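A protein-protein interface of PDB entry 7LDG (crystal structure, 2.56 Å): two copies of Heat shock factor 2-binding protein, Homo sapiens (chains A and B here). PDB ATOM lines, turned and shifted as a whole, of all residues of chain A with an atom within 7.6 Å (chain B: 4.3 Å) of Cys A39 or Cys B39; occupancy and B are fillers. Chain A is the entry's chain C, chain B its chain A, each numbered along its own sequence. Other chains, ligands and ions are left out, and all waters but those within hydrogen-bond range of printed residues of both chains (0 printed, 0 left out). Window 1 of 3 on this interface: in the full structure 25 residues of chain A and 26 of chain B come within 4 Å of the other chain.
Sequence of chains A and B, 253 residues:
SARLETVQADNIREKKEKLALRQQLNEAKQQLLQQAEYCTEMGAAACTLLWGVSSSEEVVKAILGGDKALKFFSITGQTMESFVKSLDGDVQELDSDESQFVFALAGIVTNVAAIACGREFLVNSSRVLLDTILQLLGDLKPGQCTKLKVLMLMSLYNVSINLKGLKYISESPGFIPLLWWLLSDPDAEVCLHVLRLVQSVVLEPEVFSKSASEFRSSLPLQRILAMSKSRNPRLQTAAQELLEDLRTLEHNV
Tyr B38 touches Ile A75 (O to CD1, 3.7 Å). Ile A75 touches Glu B41 (CD1 to CB, 3.999 Å). CD1 of Ile A75 touches N of Met B42 (3.7 Å).
Of chain B, only Cys B39 comes within 4 Å of Cys A39. Cys B39 touches just one residue of chain A: Cys A39. Of the printed residues of chain A, Tyr B38 touches Ile A75. Printed residues of chain A within 4 Å of Met B42: Ile A75 (3.7 Å). Of the printed residues of chain A, Glu B41 touches Ile A75 (3.999 Å). Printed residues of chain B within 4 Å of Ile A75: Tyr B38 (3.7 Å), Glu B41 (3.999 Å) and Met B42 (3.7 Å). Gln A34 touches none of the printed residues of chain B. The nearest printed residue of chain B that does not touch Cys A39 is Gln B35 (5.0 Å). The nearest residue of chain A that does not touch Cys B39 is Gln A35 (5.3 Å).
SG of Cys B39 forms a disulfide with SG of Cys A39, at 2.0 Å.
Of the 9 printed residues of chain B, 4 touch a printed residue of chain A. Printed residues of chain B that touch a printed residue of chain A: Tyr B38, Cys B39, Glu B41 and Met B42. Among the printed residues, 4 pairs touch across the chains.
O of Ile A75 lies within hydrogen-bond range of OG1 of Thr A79, at 3.2 Å.
Cys B39 touches its own counterpart, Cys A39. Positions printed for both chains: 35, 36, 37, 38, 39, 40, 41, 42 and 43.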
ATOM      1  N   LEU A  33      10.027  -3.926  -8.992  1.00  0.00           N
ATOM      2  CA  LEU A  33      11.185  -4.280  -8.181  1.00  0.00           C
ATOM      3  C   LEU A  33      12.488  -3.999  -8.920  1.00  0.00           C
ATOM      4  O   LEU A  33      13.477  -3.581  -8.304  1.00  0.00           O
ATOM      5  CB  LEU A  33      11.101  -5.751  -7.777  1.00  0.00           C
ATOM      6  CG  LEU A  33      12.292  -6.329  -7.011  1.00  0.00           C
ATOM      7  CD1 LEU A  33      12.400  -5.710  -5.624  1.00  0.00           C
ATOM      8  CD2 LEU A  33      12.188  -7.844  -6.926  1.00  0.00           C
ATOM      9  N   GLN A  34      12.511  -4.222 -10.237  1.00  0.00           N
ATOM     10  CA  GLN A  34      13.732  -3.996 -11.004  1.00  0.00           C
ATOM     11  C   GLN A  34      14.083  -2.513 -11.050  1.00  0.00           C
ATOM     12  O   GLN A  34      15.258  -2.145 -10.972  1.00  0.00           O
ATOM     13  CB  GLN A  34      13.574  -4.554 -12.419  1.00  0.00           C
ATOM     14  CG  GLN A  34      14.781  -4.330 -13.325  1.00  0.00           C
ATOM     15  CD  GLN A  34      15.982  -5.167 -12.927  1.00  0.00           C
ATOM     16  OE1 GLN A  34      15.908  -6.396 -12.878  1.00  0.00           O
ATOM     17  NE2 GLN A  34      17.096  -4.505 -12.638  1.00  0.00           N
ATOM     18  N   GLN A  35      13.073  -1.646 -11.176  1.00  0.00           N
ATOM     19  CA  GLN A  35      13.319  -0.209 -11.126  1.00  0.00           C
ATOM     20  C   GLN A  35      13.870   0.206  -9.772  1.00  0.00           C
ATOM     21  O   GLN A  35      14.805   1.010  -9.696  1.00  0.00           O
ATOM     22  CB  GLN A  35      12.034   0.560 -11.427  1.00  0.00           C
ATOM     23  CG  GLN A  35      11.738   0.739 -12.893  1.00  0.00           C
ATOM     24  CD  GLN A  35      10.676   1.794 -13.127  1.00  0.00           C
ATOM     25  OE1 GLN A  35      10.231   2.462 -12.190  1.00  0.00           O
ATOM     26  NE2 GLN A  35      10.265   1.955 -14.379  1.00  0.00           N
ATOM     27  N   ALA A  36      13.288  -0.317  -8.690  1.00  0.00           N
ATOM     28  CA  ALA A  36      13.774   0.011  -7.353  1.00  0.00           C
ATOM     29  C   ALA A  36      15.242  -0.362  -7.191  1.00  0.00           C
ATOM     30  O   ALA A  36      16.015   0.382  -6.575  1.00  0.00           O
ATOM     31  CB  ALA A  36      12.923  -0.693  -6.298  1.00  0.00           C
ATOM     32  N   GLU A  37      15.648  -1.509  -7.740  1.00  0.00           N
ATOM     33  CA  GLU A  37      17.044  -1.920  -7.649  1.00  0.00           C
ATOM     34  C   GLU A  37      17.939  -1.009  -8.475  1.00  0.00           C
ATOM     35  O   GLU A  37      18.999  -0.574  -8.011  1.00  0.00           O
ATOM     36  CB  GLU A  37      17.197  -3.369  -8.104  1.00  0.00           C
ATOM     37  CG  GLU A  37      18.639  -3.840  -8.161  1.00  0.00           C
ATOM     38  CD  GLU A  37      18.763  -5.263  -8.659  1.00  0.00           C
ATOM     39  OE1 GLU A  37      17.745  -5.821  -9.120  1.00  0.00           O
ATOM     40  OE2 GLU A  37      19.876  -5.826  -8.588  1.00  0.00           O
ATOM     41  N   TYR A  38      17.531  -0.718  -9.709  1.00  0.00           N
ATOM     42  CA  TYR A  38      18.308   0.188 -10.542  1.00  0.00           C
ATOM     43  C   TYR A  38      18.369   1.587  -9.943  1.00  0.00           C
ATOM     44  O   TYR A  38      19.331   2.323 -10.183  1.00  0.00           O
ATOM     45  CB  TYR A  38      17.708   0.241 -11.943  1.00  0.00           C
ATOM     46  CG  TYR A  38      18.456   1.145 -12.883  1.00  0.00           C
ATOM     47  CD1 TYR A  38      19.530   0.667 -13.619  1.00  0.00           C
ATOM     48  CD2 TYR A  38      18.093   2.480 -13.033  1.00  0.00           C
ATOM     49  CE1 TYR A  38      20.218   1.485 -14.484  1.00  0.00           C
ATOM     50  CE2 TYR A  38      18.782   3.312 -13.890  1.00  0.00           C
ATOM     51  CZ  TYR A  38      19.846   2.805 -14.609  1.00  0.00           C
ATOM     52  OH  TYR A  38      20.543   3.608 -15.467  1.00  0.00           O
ATOM     53  N   CYS A  39      17.357   1.969  -9.162  1.00  0.00           N
ATOM     54  CA  CYS A  39      17.311   3.314  -8.604  1.00  0.00           C
ATOM     55  C   CYS A  39      18.295   3.468  -7.448  1.00  0.00           C
ATOM     56  O   CYS A  39      19.138   4.371  -7.455  1.00  0.00           O
ATOM     57  CB  CYS A  39      15.886   3.648  -8.157  1.00  0.00           C
ATOM     58  SG  CYS A  39      15.669   5.405  -7.827  1.00  0.00           S
ATOM     59  N   THR A  40      18.205   2.591  -6.444  1.00  0.00           N
ATOM     60  CA  THR A  40      19.143   2.664  -5.330  1.00  0.00           C
ATOM     61  C   THR A  40      20.566   2.307  -5.741  1.00  0.00           C
ATOM     62  O   THR A  40      21.496   2.553  -4.968  1.00  0.00           O
ATOM     63  CB  THR A  40      18.691   1.751  -4.187  1.00  0.00           C
ATOM     64  OG1 THR A  40      19.098   0.404  -4.454  1.00  0.00           O
ATOM     65  CG2 THR A  40      17.176   1.797  -4.028  1.00  0.00           C
ATOM     66  N   GLU A  41      20.753   1.734  -6.931  1.00  0.00           N
ATOM     67  CA  GLU A  41      22.090   1.465  -7.448  1.00  0.00           C
ATOM     68  C   GLU A  41      22.741   2.739  -7.970  1.00  0.00           C
ATOM     69  O   GLU A  41      23.935   2.969  -7.751  1.00  0.00           O
ATOM     70  CB  GLU A  41      22.009   0.403  -8.546  1.00  0.00           C
ATOM     71  CG  GLU A  41      23.340  -0.099  -9.079  1.00  0.00           C
ATOM     72  CD  GLU A  41      23.166  -1.244 -10.066  1.00  0.00           C
ATOM     73  OE1 GLU A  41      22.087  -1.871 -10.063  1.00  0.00           O
ATOM     74  OE2 GLU A  41      24.102  -1.518 -10.846  1.00  0.00           O
ATOM     75  N   MET A  42      21.973   3.577  -8.659  1.00  0.00           N
ATOM     76  CA  MET A  42      22.464   4.875  -9.111  1.00  0.00           C
ATOM     77  C   MET A  42      22.585   5.827  -7.921  1.00  0.00           C
ATOM     78  O   MET A  42      23.515   6.633  -7.845  1.00  0.00           O
ATOM     79  CB  MET A  42      21.538   5.461 -10.186  1.00  0.00           C
ATOM     80  CG  MET A  42      21.781   6.936 -10.513  1.00  0.00           C
ATOM     81  SD  MET A  42      23.546   7.353 -11.272  1.00  0.00           S
ATOM     82  CE  MET A  42      23.194   7.065 -13.166  1.00  0.00           C
ATOM     83  N   GLY A  43      21.641   5.717  -6.985  1.00  0.00           N
ATOM     84  CA  GLY A  43      21.694   6.555  -5.800  1.00  0.00           C
ATOM     85  C   GLY A  43      22.938   6.304  -4.970  1.00  0.00           C
ATOM     86  O   GLY A  43      23.633   7.239  -4.565  1.00  0.00           O
ATOM     87  N   ALA A  44      23.240   5.030  -4.713  1.00  0.00           N
ATOM     88  CA  ALA A  44      24.435   4.698  -3.945  1.00  0.00           C
ATOM     89  C   ALA A  44      25.697   5.154  -4.666  1.00  0.00           C
ATOM     90  O   ALA A  44      26.633   5.654  -4.035  1.00  0.00           O
ATOM     91  CB  ALA A  44      24.484   3.194  -3.671  1.00  0.00           C
ATOM     92  N   ALA A  45      25.732   5.007  -5.988  1.00  0.00           N
ATOM     93  CA  ALA A  45      26.928   5.374  -6.737  1.00  0.00           C
ATOM     94  C   ALA A  45      27.130   6.883  -6.748  1.00  0.00           C
ATOM     95  O   ALA A  45      28.225   7.375  -6.453  1.00  0.00           O
ATOM     96  CB  ALA A  45      26.840   4.829  -8.164  1.00  0.00           C
ATOM     97  N   ILE A  75      14.991  16.218  -0.869  1.00  0.00           N
ATOM     98  CA  ILE A  75      14.754  14.815  -1.195  1.00  0.00           C
ATOM     99  C   ILE A  75      15.699  13.896  -0.425  1.00  0.00           C
ATOM    100  O   ILE A  75      15.379  12.718  -0.216  1.00  0.00           O
ATOM    101  CB  ILE A  75      14.850  14.599  -2.721  1.00  0.00           C
ATOM    102  CG1 ILE A  75      14.457  13.166  -3.088  1.00  0.00           C
ATOM    103  CG2 ILE A  75      16.243  14.928  -3.232  1.00  0.00           C
ATOM    104  CD1 ILE A  75      14.177  12.963  -4.552  1.00  0.00           C
ATOM    105  N   THR A  79      14.137  10.429   1.144  1.00  0.00           N
ATOM    106  CA  THR A  79      14.616   9.073   0.897  1.00  0.00           C
ATOM    107  C   THR A  79      15.254   8.467   2.141  1.00  0.00           C
ATOM    108  O   THR A  79      15.222   7.243   2.318  1.00  0.00           O
ATOM    109  CB  THR A  79      15.601   9.069  -0.275  1.00  0.00           C
ATOM    110  OG1 THR A  79      16.746   9.857   0.062  1.00  0.00           O
ATOM    111  CG2 THR A  79      14.953   9.664  -1.516  1.00  0.00           C
ATOM    112  N   PHE A  83      13.550   4.919   3.594  1.00  0.00           N
ATOM    113  CA  PHE A  83      14.217   3.629   3.733  1.00  0.00           C
ATOM    114  C   PHE A  83      14.160   3.114   5.167  1.00  0.00           C
ATOM    115  O   PHE A  83      13.979   1.913   5.389  1.00  0.00           O
ATOM    116  CB  PHE A  83      15.663   3.731   3.251  1.00  0.00           C
ATOM    117  CG  PHE A  83      15.809   3.641   1.756  1.00  0.00           C
ATOM    118  CD1 PHE A  83      14.755   3.201   0.970  1.00  0.00           C
ATOM    119  CD2 PHE A  83      17.001   3.985   1.139  1.00  0.00           C
ATOM    120  CE1 PHE A  83      14.888   3.113  -0.406  1.00  0.00           C
ATOM    121  CE2 PHE A  83      17.140   3.899  -0.236  1.00  0.00           C
ATOM    122  CZ  PHE A  83      16.083   3.462  -1.009  1.00  0.00           C
ATOM    123  N   PHE A 101      23.477   3.777   0.186  1.00  0.00           N
ATOM    124  CA  PHE A 101      22.728   4.960  -0.222  1.00  0.00           C
ATOM    125  C   PHE A 101      22.475   5.878   0.970  1.00  0.00           C
ATOM    126  O   PHE A 101      22.861   7.053   0.963  1.00  0.00           O
ATOM    127  CB  PHE A 101      21.410   4.522  -0.868  1.00  0.00           C
ATOM    128  CG  PHE A 101      20.741   5.581  -1.703  1.00  0.00           C
ATOM    129  CD1 PHE A 101      21.258   6.865  -1.789  1.00  0.00           C
ATOM    130  CD2 PHE A 101      19.583   5.284  -2.401  1.00  0.00           C
ATOM    131  CE1 PHE A 101      20.629   7.830  -2.558  1.00  0.00           C
ATOM    132  CE2 PHE A 101      18.950   6.241  -3.171  1.00  0.00           C
ATOM    133  CZ  PHE A 101      19.474   7.517  -3.249  1.00  0.00           C
ATOM    134  N   GLN B  35       7.480   6.126  -8.448  1.00  0.00           N
ATOM    135  CA  GLN B  35       8.867   5.767  -8.173  1.00  0.00           C
ATOM    136  C   GLN B  35       9.813   6.361  -9.206  1.00  0.00           C
ATOM    137  O   GLN B  35      10.933   6.751  -8.862  1.00  0.00           O
ATOM    138  CB  GLN B  35       9.020   4.251  -8.125  1.00  0.00           C
ATOM    139  CG  GLN B  35       8.537   3.638  -6.826  1.00  0.00           C
ATOM    140  CD  GLN B  35       8.738   2.144  -6.780  1.00  0.00           C
ATOM    141  OE1 GLN B  35       9.578   1.596  -7.499  1.00  0.00           O
ATOM    142  NE2 GLN B  35       7.962   1.470  -5.938  1.00  0.00           N
ATOM    143  N   ALA B  36       9.385   6.439 -10.467  1.00  0.00           N
ATOM    144  CA  ALA B  36      10.257   6.972 -11.507  1.00  0.00           C
ATOM    145  C   ALA B  36      10.513   8.460 -11.311  1.00  0.00           C
ATOM    146  O   ALA B  36      11.650   8.922 -11.460  1.00  0.00           O
ATOM    147  CB  ALA B  36       9.653   6.704 -12.884  1.00  0.00           C
ATOM    148  N   GLU B  37       9.472   9.227 -10.971  1.00  0.00           N
ATOM    149  CA  GLU B  37       9.649  10.668 -10.828  1.00  0.00           C
ATOM    150  C   GLU B  37      10.538  11.009  -9.639  1.00  0.00           C
ATOM    151  O   GLU B  37      11.309  11.975  -9.699  1.00  0.00           O
ATOM    152  CB  GLU B  37       8.295  11.364 -10.696  1.00  0.00           C
ATOM    153  CG  GLU B  37       8.398  12.881 -10.725  1.00  0.00           C
ATOM    154  CD  GLU B  37       7.057  13.567 -10.587  1.00  0.00           C
ATOM    155  OE1 GLU B  37       6.028  12.860 -10.544  1.00  0.00           O
ATOM    156  OE2 GLU B  37       7.032  14.815 -10.520  1.00  0.00           O
ATOM    157  N   TYR B  38      10.448  10.237  -8.553  1.00  0.00           N
ATOM    158  CA  TYR B  38      11.386  10.419  -7.451  1.00  0.00           C
ATOM    159  C   TYR B  38      12.803  10.074  -7.882  1.00  0.00           C
ATOM    160  O   TYR B  38      13.753  10.795  -7.553  1.00  0.00           O
ATOM    161  CB  TYR B  38      10.977   9.560  -6.256  1.00  0.00           C
ATOM    162  CG  TYR B  38       9.910  10.177  -5.384  1.00  0.00           C
ATOM    163  CD1 TYR B  38       8.781   9.453  -5.020  1.00  0.00           C
ATOM    164  CD2 TYR B  38      10.035  11.478  -4.916  1.00  0.00           C
ATOM    165  CE1 TYR B  38       7.802  10.011  -4.220  1.00  0.00           C
ATOM    166  CE2 TYR B  38       9.059  12.045  -4.113  1.00  0.00           C
ATOM    167  CZ  TYR B  38       7.944  11.306  -3.771  1.00  0.00           C
ATOM    168  OH  TYR B  38       6.970  11.862  -2.974  1.00  0.00           O
ATOM    169  N   CYS B  39      12.959   8.979  -8.629  1.00  0.00           N
ATOM    170  CA  CYS B  39      14.287   8.533  -9.028  1.00  0.00           C
ATOM    171  C   CYS B  39      14.976   9.574  -9.901  1.00  0.00           C
ATOM    172  O   CYS B  39      16.129   9.947  -9.650  1.00  0.00           O
ATOM    173  CB  CYS B  39      14.189   7.189  -9.750  1.00  0.00           C
ATOM    174  SG  CYS B  39      15.719   6.258  -9.672  1.00  0.00           S
ATOM    175  N   THR B  40      14.281  10.065 -10.931  1.00  0.00           N
ATOM    176  CA  THR B  40      14.872  11.092 -11.781  1.00  0.00           C
ATOM    177  C   THR B  40      15.094  12.392 -11.020  1.00  0.00           C
ATOM    178  O   THR B  40      16.015  13.147 -11.348  1.00  0.00           O
ATOM    179  CB  THR B  40      13.998  11.343 -13.009  1.00  0.00           C
ATOM    180  OG1 THR B  40      12.781  11.985 -12.608  1.00  0.00           O
ATOM    181  CG2 THR B  40      13.667  10.033 -13.702  1.00  0.00           C
ATOM    182  N   GLU B  41      14.272  12.675 -10.007  1.00  0.00           N
ATOM    183  CA  GLU B  41      14.486  13.876  -9.204  1.00  0.00           C
ATOM    184  C   GLU B  41      15.777  13.773  -8.404  1.00  0.00           C
ATOM    185  O   GLU B  41      16.597  14.698  -8.405  1.00  0.00           O
ATOM    186  CB  GLU B  41      13.294  14.113  -8.279  1.00  0.00           C
ATOM    187  CG  GLU B  41      12.283  15.104  -8.827  1.00  0.00           C
ATOM    188  CD  GLU B  41      11.029  15.192  -7.980  1.00  0.00           C
ATOM    189  OE1 GLU B  41      11.010  14.606  -6.875  1.00  0.00           O
ATOM    190  OE2 GLU B  41      10.060  15.846  -8.423  1.00  0.00           O
ATOM    191  N   MET B  42      15.975  12.653  -7.719  1.00  0.00           N
ATOM    192  CA  MET B  42      17.215  12.409  -6.998  1.00  0.00           C
ATOM    193  C   MET B  42      18.396  12.389  -7.964  1.00  0.00           C
ATOM    194  O   MET B  42      19.431  13.013  -7.715  1.00  0.00           O
ATOM    195  CB  MET B  42      17.150  11.091  -6.224  1.00  0.00           C
ATOM    196  CG  MET B  42      18.458  10.709  -5.526  1.00  0.00           C
ATOM    197  SD  MET B  42      18.879  11.744  -3.910  1.00  0.00           S
ATOM    198  CE  MET B  42      19.661  13.301  -4.724  1.00  0.00           C
ATOM    199  N   GLY B  43      18.228  11.675  -9.079  1.00  0.00           N
ATOM    200  CA  GLY B  43      19.287  11.628 -10.073  1.00  0.00           C
ATOM    201  C   GLY B  43      19.659  13.001 -10.594  1.00  0.00           C
ATOM    202  O   GLY B  43      20.841  13.336 -10.697  1.00  0.00           O
